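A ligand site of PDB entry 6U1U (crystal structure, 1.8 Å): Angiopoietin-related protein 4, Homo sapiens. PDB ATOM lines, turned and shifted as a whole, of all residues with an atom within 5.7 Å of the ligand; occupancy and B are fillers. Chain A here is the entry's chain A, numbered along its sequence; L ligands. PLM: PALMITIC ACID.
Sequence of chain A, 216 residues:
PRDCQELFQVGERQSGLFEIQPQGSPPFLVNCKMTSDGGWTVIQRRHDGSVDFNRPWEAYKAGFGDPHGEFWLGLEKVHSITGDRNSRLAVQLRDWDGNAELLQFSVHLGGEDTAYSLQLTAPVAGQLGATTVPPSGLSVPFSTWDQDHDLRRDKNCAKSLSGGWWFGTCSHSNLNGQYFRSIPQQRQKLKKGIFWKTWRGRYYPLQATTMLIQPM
The backbone NH (N) of His 172 lies within hydrogen-bond range of the side-chain hydroxyl (OG1) of Thr 169 (3.2 Å). OG1 of Thr 169 sits at hydrogen-bond distance from N of Ser 171. The backbone carbonyl oxygen of His 172 sits at hydrogen-bond distance from the backbone NH of Lys 197 (2.9 Å). The side-chain amino group (NZ) of Lys 197 is in hydrogen-bond range of the backbone carbonyl oxygen (O) of Ser 171. N of Leu 89 sits at hydrogen-bond distance from O of Phe 105, 2.8 Å away. A ring nitrogen (NE2) of His 172 lies within hydrogen-bond range of the backbone carbonyl oxygen of Leu 128, at 3.1 Å. N of Val 140 sits at hydrogen-bond distance from O of Leu 118 (2.8 Å). A ring nitrogen (ND1) of His 172 is in hydrogen-bond range of the side-chain hydroxyl of Ser 173, 2.7 Å away.
Merely in contact with the ligand: Leu 89 (3.3 Å), Phe 105 (3.4 Å), Trp 166 (3.4 Å), Leu 128 (3.5 Å), Leu 118 (3.6 Å), Trp 196 (3.6 Å), His 172 (3.6 Å), Ser 171 (3.7 Å) and Val 107 (3.8 Å). 11 residues have an atom within 4 Å of the ligand: Leu 89, Phe 105, Val 107, Leu 118, Leu 128, Trp 166, Thr 169, Ser 171, His 172, Trp 196 and Lys 197. Along chain A the residues within 4 Å of the ligand span positions 89 to 197.
The side-chain hydroxyl (OG1) of Thr 169 sits at hydrogen-bond distance from an oxygen (O1) of the ligand, at 2.8 Å. An oxygen (O1) of the ligand is in salt-bridge range of the side-chain amino group (NZ) of Lys 197 (3.1 Å).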
ATOM      1  N   LEU A  89     -24.483 -27.403 -20.057  1.00  0.00           N
ATOM      2  CA  LEU A  89     -24.490 -27.737 -21.496  1.00  0.00           C
ATOM      3  C   LEU A  89     -23.062 -28.094 -21.896  1.00  0.00           C
ATOM      4  O   LEU A  89     -22.246 -27.257 -21.808  1.00  0.00           O
ATOM      5  CB  LEU A  89     -24.980 -26.540 -22.315  1.00  0.00           C
ATOM      6  CG  LEU A  89     -24.976 -26.709 -23.818  1.00  0.00           C
ATOM      7  CD1 LEU A  89     -25.767 -27.923 -24.231  1.00  0.00           C
ATOM      8  CD2 LEU A  89     -25.552 -25.489 -24.505  1.00  0.00           C
ATOM      9  N   VAL A  91     -20.344 -29.228 -24.744  1.00  0.00           N
ATOM     10  CA  VAL A  91     -20.173 -29.135 -26.189  1.00  0.00           C
ATOM     11  C   VAL A  91     -18.860 -29.819 -26.501  1.00  0.00           C
ATOM     12  O   VAL A  91     -17.823 -29.433 -25.957  1.00  0.00           O
ATOM     13  CB  VAL A  91     -20.157 -27.674 -26.657  1.00  0.00           C
ATOM     14  CG1 VAL A  91     -19.816 -27.603 -28.160  1.00  0.00           C
ATOM     15  CG2 VAL A  91     -21.525 -26.994 -26.390  1.00  0.00           C
ATOM     16  N   PHE A 105     -20.767 -25.189 -20.331  1.00  0.00           N
ATOM     17  CA  PHE A 105     -21.299 -23.866 -19.970  1.00  0.00           C
ATOM     18  C   PHE A 105     -22.575 -24.046 -19.163  1.00  0.00           C
ATOM     19  O   PHE A 105     -23.318 -24.932 -19.465  1.00  0.00           O
ATOM     20  CB  PHE A 105     -21.703 -23.083 -21.226  1.00  0.00           C
ATOM     21  CG  PHE A 105     -20.638 -22.969 -22.277  1.00  0.00           C
ATOM     22  CD1 PHE A 105     -19.683 -21.992 -22.196  1.00  0.00           C
ATOM     23  CD2 PHE A 105     -20.573 -23.864 -23.311  1.00  0.00           C
ATOM     24  CE1 PHE A 105     -18.687 -21.890 -23.147  1.00  0.00           C
ATOM     25  CE2 PHE A 105     -19.573 -23.774 -24.252  1.00  0.00           C
ATOM     26  CZ  PHE A 105     -18.632 -22.788 -24.165  1.00  0.00           C
ATOM     27  N   VAL A 107     -26.254 -22.876 -18.570  1.00  0.00           N
ATOM     28  CA  VAL A 107     -27.276 -22.168 -19.354  1.00  0.00           C
ATOM     29  C   VAL A 107     -28.641 -22.342 -18.714  1.00  0.00           C
ATOM     30  O   VAL A 107     -28.876 -23.262 -17.929  1.00  0.00           O
ATOM     31  CB  VAL A 107     -27.343 -22.662 -20.827  1.00  0.00           C
ATOM     32  CG1 VAL A 107     -25.955 -22.598 -21.477  1.00  0.00           C
ATOM     33  CG2 VAL A 107     -27.873 -24.111 -20.891  1.00  0.00           C
ATOM     34  N   LEU A 118     -31.609 -19.576 -25.671  1.00  0.00           N
ATOM     35  CA  LEU A 118     -30.540 -19.863 -24.723  1.00  0.00           C
ATOM     36  C   LEU A 118     -30.327 -18.597 -23.918  1.00  0.00           C
ATOM     37  O   LEU A 118     -30.165 -17.505 -24.496  1.00  0.00           O
ATOM     38  CB  LEU A 118     -29.276 -20.249 -25.446  1.00  0.00           C
ATOM     39  CG  LEU A 118     -28.339 -21.305 -24.892  1.00  0.00           C
ATOM     40  CD1 LEU A 118     -29.096 -22.552 -24.457  1.00  0.00           C
ATOM     41  CD2 LEU A 118     -27.348 -21.619 -26.018  1.00  0.00           C
ATOM     42  N   LEU A 120     -28.155 -16.763 -21.171  1.00  0.00           N
ATOM     43  CA  LEU A 120     -26.802 -16.801 -20.617  1.00  0.00           C
ATOM     44  C   LEU A 120     -26.596 -15.688 -19.590  1.00  0.00           C
ATOM     45  O   LEU A 120     -26.980 -14.591 -19.838  1.00  0.00           O
ATOM     46  CB  LEU A 120     -25.822 -16.641 -21.777  1.00  0.00           C
ATOM     47  CG  LEU A 120     -25.980 -17.639 -22.916  1.00  0.00           C
ATOM     48  CD1 LEU A 120     -24.998 -17.356 -24.026  1.00  0.00           C
ATOM     49  CD2 LEU A 120     -25.786 -19.037 -22.407  1.00  0.00           C
ATOM     50  N   VAL A 124     -21.001 -16.154 -18.437  1.00  0.00           N
ATOM     51  CA  VAL A 124     -21.017 -17.233 -19.429  1.00  0.00           C
ATOM     52  C   VAL A 124     -20.937 -16.661 -20.848  1.00  0.00           C
ATOM     53  O   VAL A 124     -20.202 -17.179 -21.707  1.00  0.00           O
ATOM     54  CB  VAL A 124     -22.249 -18.125 -19.217  1.00  0.00           C
ATOM     55  CG1 VAL A 124     -22.376 -19.123 -20.350  1.00  0.00           C
ATOM     56  CG2 VAL A 124     -22.131 -18.860 -17.859  1.00  0.00           C
ATOM     57  N   ALA A 125     -21.707 -15.607 -21.130  1.00  0.00           N
ATOM     58  CA  ALA A 125     -21.566 -14.953 -22.425  1.00  0.00           C
ATOM     59  C   ALA A 125     -20.129 -14.529 -22.641  1.00  0.00           C
ATOM     60  O   ALA A 125     -19.622 -14.579 -23.780  1.00  0.00           O
ATOM     61  CB  ALA A 125     -22.505 -13.749 -22.515  1.00  0.00           C
ATOM     62  N   LEU A 128     -18.010 -17.234 -23.926  1.00  0.00           N
ATOM     63  CA  LEU A 128     -18.282 -17.518 -25.320  1.00  0.00           C
ATOM     64  C   LEU A 128     -17.730 -16.445 -26.242  1.00  0.00           C
ATOM     65  O   LEU A 128     -17.839 -16.571 -27.461  1.00  0.00           O
ATOM     66  CB  LEU A 128     -19.790 -17.702 -25.542  1.00  0.00           C
ATOM     67  CG  LEU A 128     -20.415 -18.986 -24.979  1.00  0.00           C
ATOM     68  CD1 LEU A 128     -21.890 -18.819 -24.778  1.00  0.00           C
ATOM     69  CD2 LEU A 128     -20.147 -20.195 -25.916  1.00  0.00           C
ATOM     70  N   GLY A 129     -17.162 -15.369 -25.694  1.00  0.00           N
ATOM     71  CA  GLY A 129     -16.549 -14.334 -26.505  1.00  0.00           C
ATOM     72  C   GLY A 129     -17.231 -12.986 -26.485  1.00  0.00           C
ATOM     73  O   GLY A 129     -16.676 -12.032 -27.041  1.00  0.00           O
ATOM     74  N   ALA A 130     -18.412 -12.860 -25.874  1.00  0.00           N
ATOM     75  CA  ALA A 130     -19.059 -11.557 -25.820  1.00  0.00           C
ATOM     76  C   ALA A 130     -18.334 -10.673 -24.798  1.00  0.00           C
ATOM     77  O   ALA A 130     -18.036 -11.130 -23.688  1.00  0.00           O
ATOM     78  CB  ALA A 130     -20.538 -11.728 -25.445  1.00  0.00           C
ATOM     79  N   LEU A 138     -27.743 -12.353 -21.509  1.00  0.00           N
ATOM     80  CA  LEU A 138     -27.971 -12.382 -22.954  1.00  0.00           C
ATOM     81  C   LEU A 138     -28.967 -13.496 -23.240  1.00  0.00           C
ATOM     82  O   LEU A 138     -28.832 -14.582 -22.676  1.00  0.00           O
ATOM     83  CB  LEU A 138     -26.623 -12.646 -23.650  1.00  0.00           C
ATOM     84  CG  LEU A 138     -26.589 -12.886 -25.151  1.00  0.00           C
ATOM     85  CD1 LEU A 138     -27.288 -11.754 -25.892  1.00  0.00           C
ATOM     86  CD2 LEU A 138     -25.137 -13.000 -25.590  1.00  0.00           C
ATOM     87  N   VAL A 140     -30.570 -15.597 -26.548  1.00  0.00           N
ATOM     88  CA  VAL A 140     -30.362 -15.813 -27.967  1.00  0.00           C
ATOM     89  C   VAL A 140     -31.422 -16.802 -28.452  1.00  0.00           C
ATOM     90  O   VAL A 140     -31.395 -17.964 -28.050  1.00  0.00           O
ATOM     91  CB  VAL A 140     -28.956 -16.348 -28.287  1.00  0.00           C
ATOM     92  CG1 VAL A 140     -28.774 -16.491 -29.776  1.00  0.00           C
ATOM     93  CG2 VAL A 140     -27.855 -15.413 -27.718  1.00  0.00           C
ATOM     94  N   TRP A 165     -29.948 -23.128 -35.471  1.00  0.00           N
ATOM     95  CA  TRP A 165     -28.961 -22.814 -34.442  1.00  0.00           C
ATOM     96  C   TRP A 165     -29.377 -21.596 -33.648  1.00  0.00           C
ATOM     97  O   TRP A 165     -30.259 -20.831 -34.044  1.00  0.00           O
ATOM     98  CB  TRP A 165     -27.564 -22.573 -35.049  1.00  0.00           C
ATOM     99  CG  TRP A 165     -26.402 -22.636 -34.081  1.00  0.00           C
ATOM    100  CD1 TRP A 165     -25.516 -21.622 -33.774  1.00  0.00           C
ATOM    101  CD2 TRP A 165     -25.975 -23.780 -33.348  1.00  0.00           C
ATOM    102  NE1 TRP A 165     -24.573 -22.077 -32.887  1.00  0.00           N
ATOM    103  CE2 TRP A 165     -24.825 -23.395 -32.597  1.00  0.00           C
ATOM    104  CE3 TRP A 165     -26.445 -25.094 -33.242  1.00  0.00           C
ATOM    105  CZ2 TRP A 165     -24.151 -24.265 -31.744  1.00  0.00           C
ATOM    106  CZ3 TRP A 165     -25.759 -25.999 -32.413  1.00  0.00           C
ATOM    107  CH2 TRP A 165     -24.619 -25.585 -31.662  1.00  0.00           C
ATOM    108  N   TRP A 166     -28.682 -21.395 -32.519  1.00  0.00           N
ATOM    109  CA  TRP A 166     -28.789 -20.173 -31.721  1.00  0.00           C
ATOM    110  C   TRP A 166     -27.802 -19.180 -32.324  1.00  0.00           C
ATOM    111  O   TRP A 166     -26.675 -19.009 -31.856  1.00  0.00           O
ATOM    112  CB  TRP A 166     -28.461 -20.449 -30.261  1.00  0.00           C
ATOM    113  CG  TRP A 166     -29.443 -21.355 -29.578  1.00  0.00           C
ATOM    114  CD1 TRP A 166     -30.667 -21.012 -29.052  1.00  0.00           C
ATOM    115  CD2 TRP A 166     -29.257 -22.752 -29.297  1.00  0.00           C
ATOM    116  NE1 TRP A 166     -31.267 -22.135 -28.475  1.00  0.00           N
ATOM    117  CE2 TRP A 166     -30.417 -23.198 -28.619  1.00  0.00           C
ATOM    118  CE3 TRP A 166     -28.250 -23.666 -29.600  1.00  0.00           C
ATOM    119  CZ2 TRP A 166     -30.586 -24.534 -28.214  1.00  0.00           C
ATOM    120  CZ3 TRP A 166     -28.414 -25.000 -29.204  1.00  0.00           C
ATOM    121  CH2 TRP A 166     -29.579 -25.424 -28.536  1.00  0.00           C
ATOM    122  N   PHE A 167     -28.228 -18.550 -33.414  1.00  0.00           N
ATOM    123  CA  PHE A 167     -27.345 -17.656 -34.168  1.00  0.00           C
ATOM    124  C   PHE A 167     -27.277 -16.301 -33.440  1.00  0.00           C
ATOM    125  O   PHE A 167     -27.951 -15.334 -33.778  1.00  0.00           O
ATOM    126  CB  PHE A 167     -27.871 -17.518 -35.597  1.00  0.00           C
ATOM    127  CG  PHE A 167     -27.773 -18.768 -36.465  1.00  0.00           C
ATOM    128  CD1 PHE A 167     -26.553 -19.294 -36.880  1.00  0.00           C
ATOM    129  CD2 PHE A 167     -28.927 -19.399 -36.929  1.00  0.00           C
ATOM    130  CE1 PHE A 167     -26.504 -20.395 -37.685  1.00  0.00           C
ATOM    131  CE2 PHE A 167     -28.872 -20.527 -37.748  1.00  0.00           C
ATOM    132  CZ  PHE A 167     -27.655 -21.018 -38.134  1.00  0.00           C
ATOM    133  N   GLY A 168     -26.457 -16.223 -32.383  1.00  0.00           N
ATOM    134  CA  GLY A 168     -26.296 -14.940 -31.686  1.00  0.00           C
ATOM    135  C   GLY A 168     -25.604 -13.881 -32.552  1.00  0.00           C
ATOM    136  O   GLY A 168     -25.900 -12.690 -32.459  1.00  0.00           O
ATOM    137  N   THR A 169     -24.627 -14.303 -33.321  1.00  0.00           N
ATOM    138  CA  THR A 169     -24.203 -13.658 -34.548  1.00  0.00           C
ATOM    139  C   THR A 169     -24.316 -14.735 -35.632  1.00  0.00           C
ATOM    140  O   THR A 169     -24.708 -15.883 -35.363  1.00  0.00           O
ATOM    141  CB  THR A 169     -22.762 -13.151 -34.438  1.00  0.00           C
ATOM    142  OG1 THR A 169     -21.896 -14.277 -34.292  1.00  0.00           O
ATOM    143  CG2 THR A 169     -22.628 -12.230 -33.223  1.00  0.00           C
ATOM    144  N   SER A 171     -21.612 -15.633 -37.015  1.00  0.00           N
ATOM    145  CA  SER A 171     -20.183 -15.901 -37.124  1.00  0.00           C
ATOM    146  C   SER A 171     -19.561 -16.620 -35.940  1.00  0.00           C
ATOM    147  O   SER A 171     -18.337 -16.788 -35.923  1.00  0.00           O
ATOM    148  CB  SER A 171     -19.416 -14.574 -37.325  1.00  0.00           C
ATOM    149  OG  SER A 171     -19.735 -14.019 -38.591  1.00  0.00           O
ATOM    150  N   HIS A 172     -20.345 -17.008 -34.925  1.00  0.00           N
ATOM    151  CA  HIS A 172     -19.775 -17.601 -33.721  1.00  0.00           C
ATOM    152  C   HIS A 172     -19.617 -19.118 -33.846  1.00  0.00           C
ATOM    153  O   HIS A 172     -18.531 -19.681 -33.606  1.00  0.00           O
ATOM    154  CB  HIS A 172     -20.650 -17.300 -32.495  1.00  0.00           C
ATOM    155  CG  HIS A 172     -20.199 -17.997 -31.253  1.00  0.00           C
ATOM    156  ND1 HIS A 172     -20.623 -19.264 -30.899  1.00  0.00           N
ATOM    157  CD2 HIS A 172     -19.312 -17.621 -30.304  1.00  0.00           C
ATOM    158  CE1 HIS A 172     -20.015 -19.626 -29.776  1.00  0.00           C
ATOM    159  NE2 HIS A 172     -19.224 -18.632 -29.386  1.00  0.00           N
ATOM    160  N   SER A 173     -20.704 -19.790 -34.233  1.00  0.00           N
ATOM    161  CA  SER A 173     -20.727 -21.246 -34.298  1.00  0.00           C
ATOM    162  C   SER A 173     -21.985 -21.680 -35.027  1.00  0.00           C
ATOM    163  O   SER A 173     -22.932 -20.915 -35.168  1.00  0.00           O
ATOM    164  CB  SER A 173     -20.753 -21.889 -32.921  1.00  0.00           C
ATOM    165  OG  SER A 173     -21.846 -21.325 -32.178  1.00  0.00           O
ATOM    166  N   TRP A 196     -17.012 -23.936 -35.087  1.00  0.00           N
ATOM    167  CA  TRP A 196     -16.929 -23.294 -33.750  1.00  0.00           C
ATOM    168  C   TRP A 196     -15.727 -22.346 -33.885  1.00  0.00           C
ATOM    169  O   TRP A 196     -14.638 -22.814 -33.822  1.00  0.00           O
ATOM    170  CB  TRP A 196     -16.746 -24.296 -32.634  1.00  0.00           C
ATOM    171  CG  TRP A 196     -16.883 -23.722 -31.263  1.00  0.00           C
ATOM    172  CD1 TRP A 196     -15.928 -23.143 -30.514  1.00  0.00           C
ATOM    173  CD2 TRP A 196     -18.067 -23.724 -30.457  1.00  0.00           C
ATOM    174  NE1 TRP A 196     -16.415 -22.747 -29.313  1.00  0.00           N
ATOM    175  CE2 TRP A 196     -17.739 -23.087 -29.249  1.00  0.00           C
ATOM    176  CE3 TRP A 196     -19.366 -24.178 -30.650  1.00  0.00           C
ATOM    177  CZ2 TRP A 196     -18.655 -22.913 -28.227  1.00  0.00           C
ATOM    178  CZ3 TRP A 196     -20.277 -24.011 -29.639  1.00  0.00           C
ATOM    179  CH2 TRP A 196     -19.929 -23.367 -28.464  1.00  0.00           C
ATOM    180  N   LYS A 197     -15.988 -21.066 -34.046  1.00  0.00           N
ATOM    181  CA  LYS A 197     -14.963 -20.148 -34.560  1.00  0.00           C
ATOM    182  C   LYS A 197     -13.741 -20.113 -33.666  1.00  0.00           C
ATOM    183  O   LYS A 197     -12.600 -20.234 -34.146  1.00  0.00           O
ATOM    184  CB  LYS A 197     -15.554 -18.759 -34.737  1.00  0.00           C
ATOM    185  CG  LYS A 197     -14.483 -17.725 -35.259  1.00  0.00           C
ATOM    186  CD  LYS A 197     -15.150 -16.447 -35.679  1.00  0.00           C
ATOM    187  CE  LYS A 197     -15.502 -15.589 -34.467  1.00  0.00           C
ATOM    188  NZ  LYS A 197     -16.477 -14.487 -34.787  1.00  0.00           N
ATOM    189  N   MET A 211     -23.428 -32.665 -28.256  1.00  0.00           N
ATOM    190  CA  MET A 211     -23.915 -31.725 -27.245  1.00  0.00           C
ATOM    191  C   MET A 211     -24.704 -32.496 -26.198  1.00  0.00           C
ATOM    192  O   MET A 211     -25.521 -33.366 -26.552  1.00  0.00           O
ATOM    193  CB  MET A 211     -24.808 -30.633 -27.873  1.00  0.00           C
ATOM    194  CG  MET A 211     -24.108 -29.917 -29.030  1.00  0.00           C
ATOM    195  SD  MET A 211     -25.229 -28.758 -29.858  1.00  0.00           S
ATOM    196  CE  MET A 211     -25.314 -27.562 -28.535  1.00  0.00           C
HETATM  197  C1  PLM L   1     -18.970 -13.803 -32.361  1.00  0.00           C
HETATM  198  O1  PLM L   1     -19.281 -13.796 -33.576  1.00  0.00           O
HETATM  199  O2  PLM L   1     -17.854 -14.112 -31.944  1.00  0.00           O
HETATM  200  C2  PLM L   1     -20.013 -13.337 -31.351  1.00  0.00           C
HETATM  201  C3  PLM L   1     -20.035 -13.939 -29.975  1.00  0.00           C
HETATM  202  C4  PLM L   1     -21.450 -14.058 -29.424  1.00  0.00           C
HETATM  203  C5  PLM L   1     -21.672 -15.125 -28.392  1.00  0.00           C
HETATM  204  C6  PLM L   1     -23.077 -15.683 -28.328  1.00  0.00           C
HETATM  205  C7  PLM L   1     -23.158 -17.110 -27.844  1.00  0.00           C
HETATM  206  C8  PLM L   1     -24.386 -17.897 -28.255  1.00  0.00           C
HETATM  207  C9  PLM L   1     -24.165 -18.709 -29.475  1.00  0.00           C
HETATM  208  CA  PLM L   1     -24.612 -20.109 -29.398  1.00  0.00           C
HETATM  209  CB  PLM L   1     -23.843 -20.984 -28.491  1.00  0.00           C
HETATM  210  CC  PLM L   1     -24.579 -22.228 -28.172  1.00  0.00           C
HETATM  211  CD  PLM L   1     -23.770 -23.298 -27.577  1.00  0.00           C
HETATM  212  CE  PLM L   1     -22.881 -22.814 -26.499  1.00  0.00           C
HETATM  213  CF  PLM L   1     -23.324 -23.080 -25.119  1.00  0.00           C
HETATM  214  CG  PLM L   1     -23.688 -21.841 -24.373  1.00  0.00           C
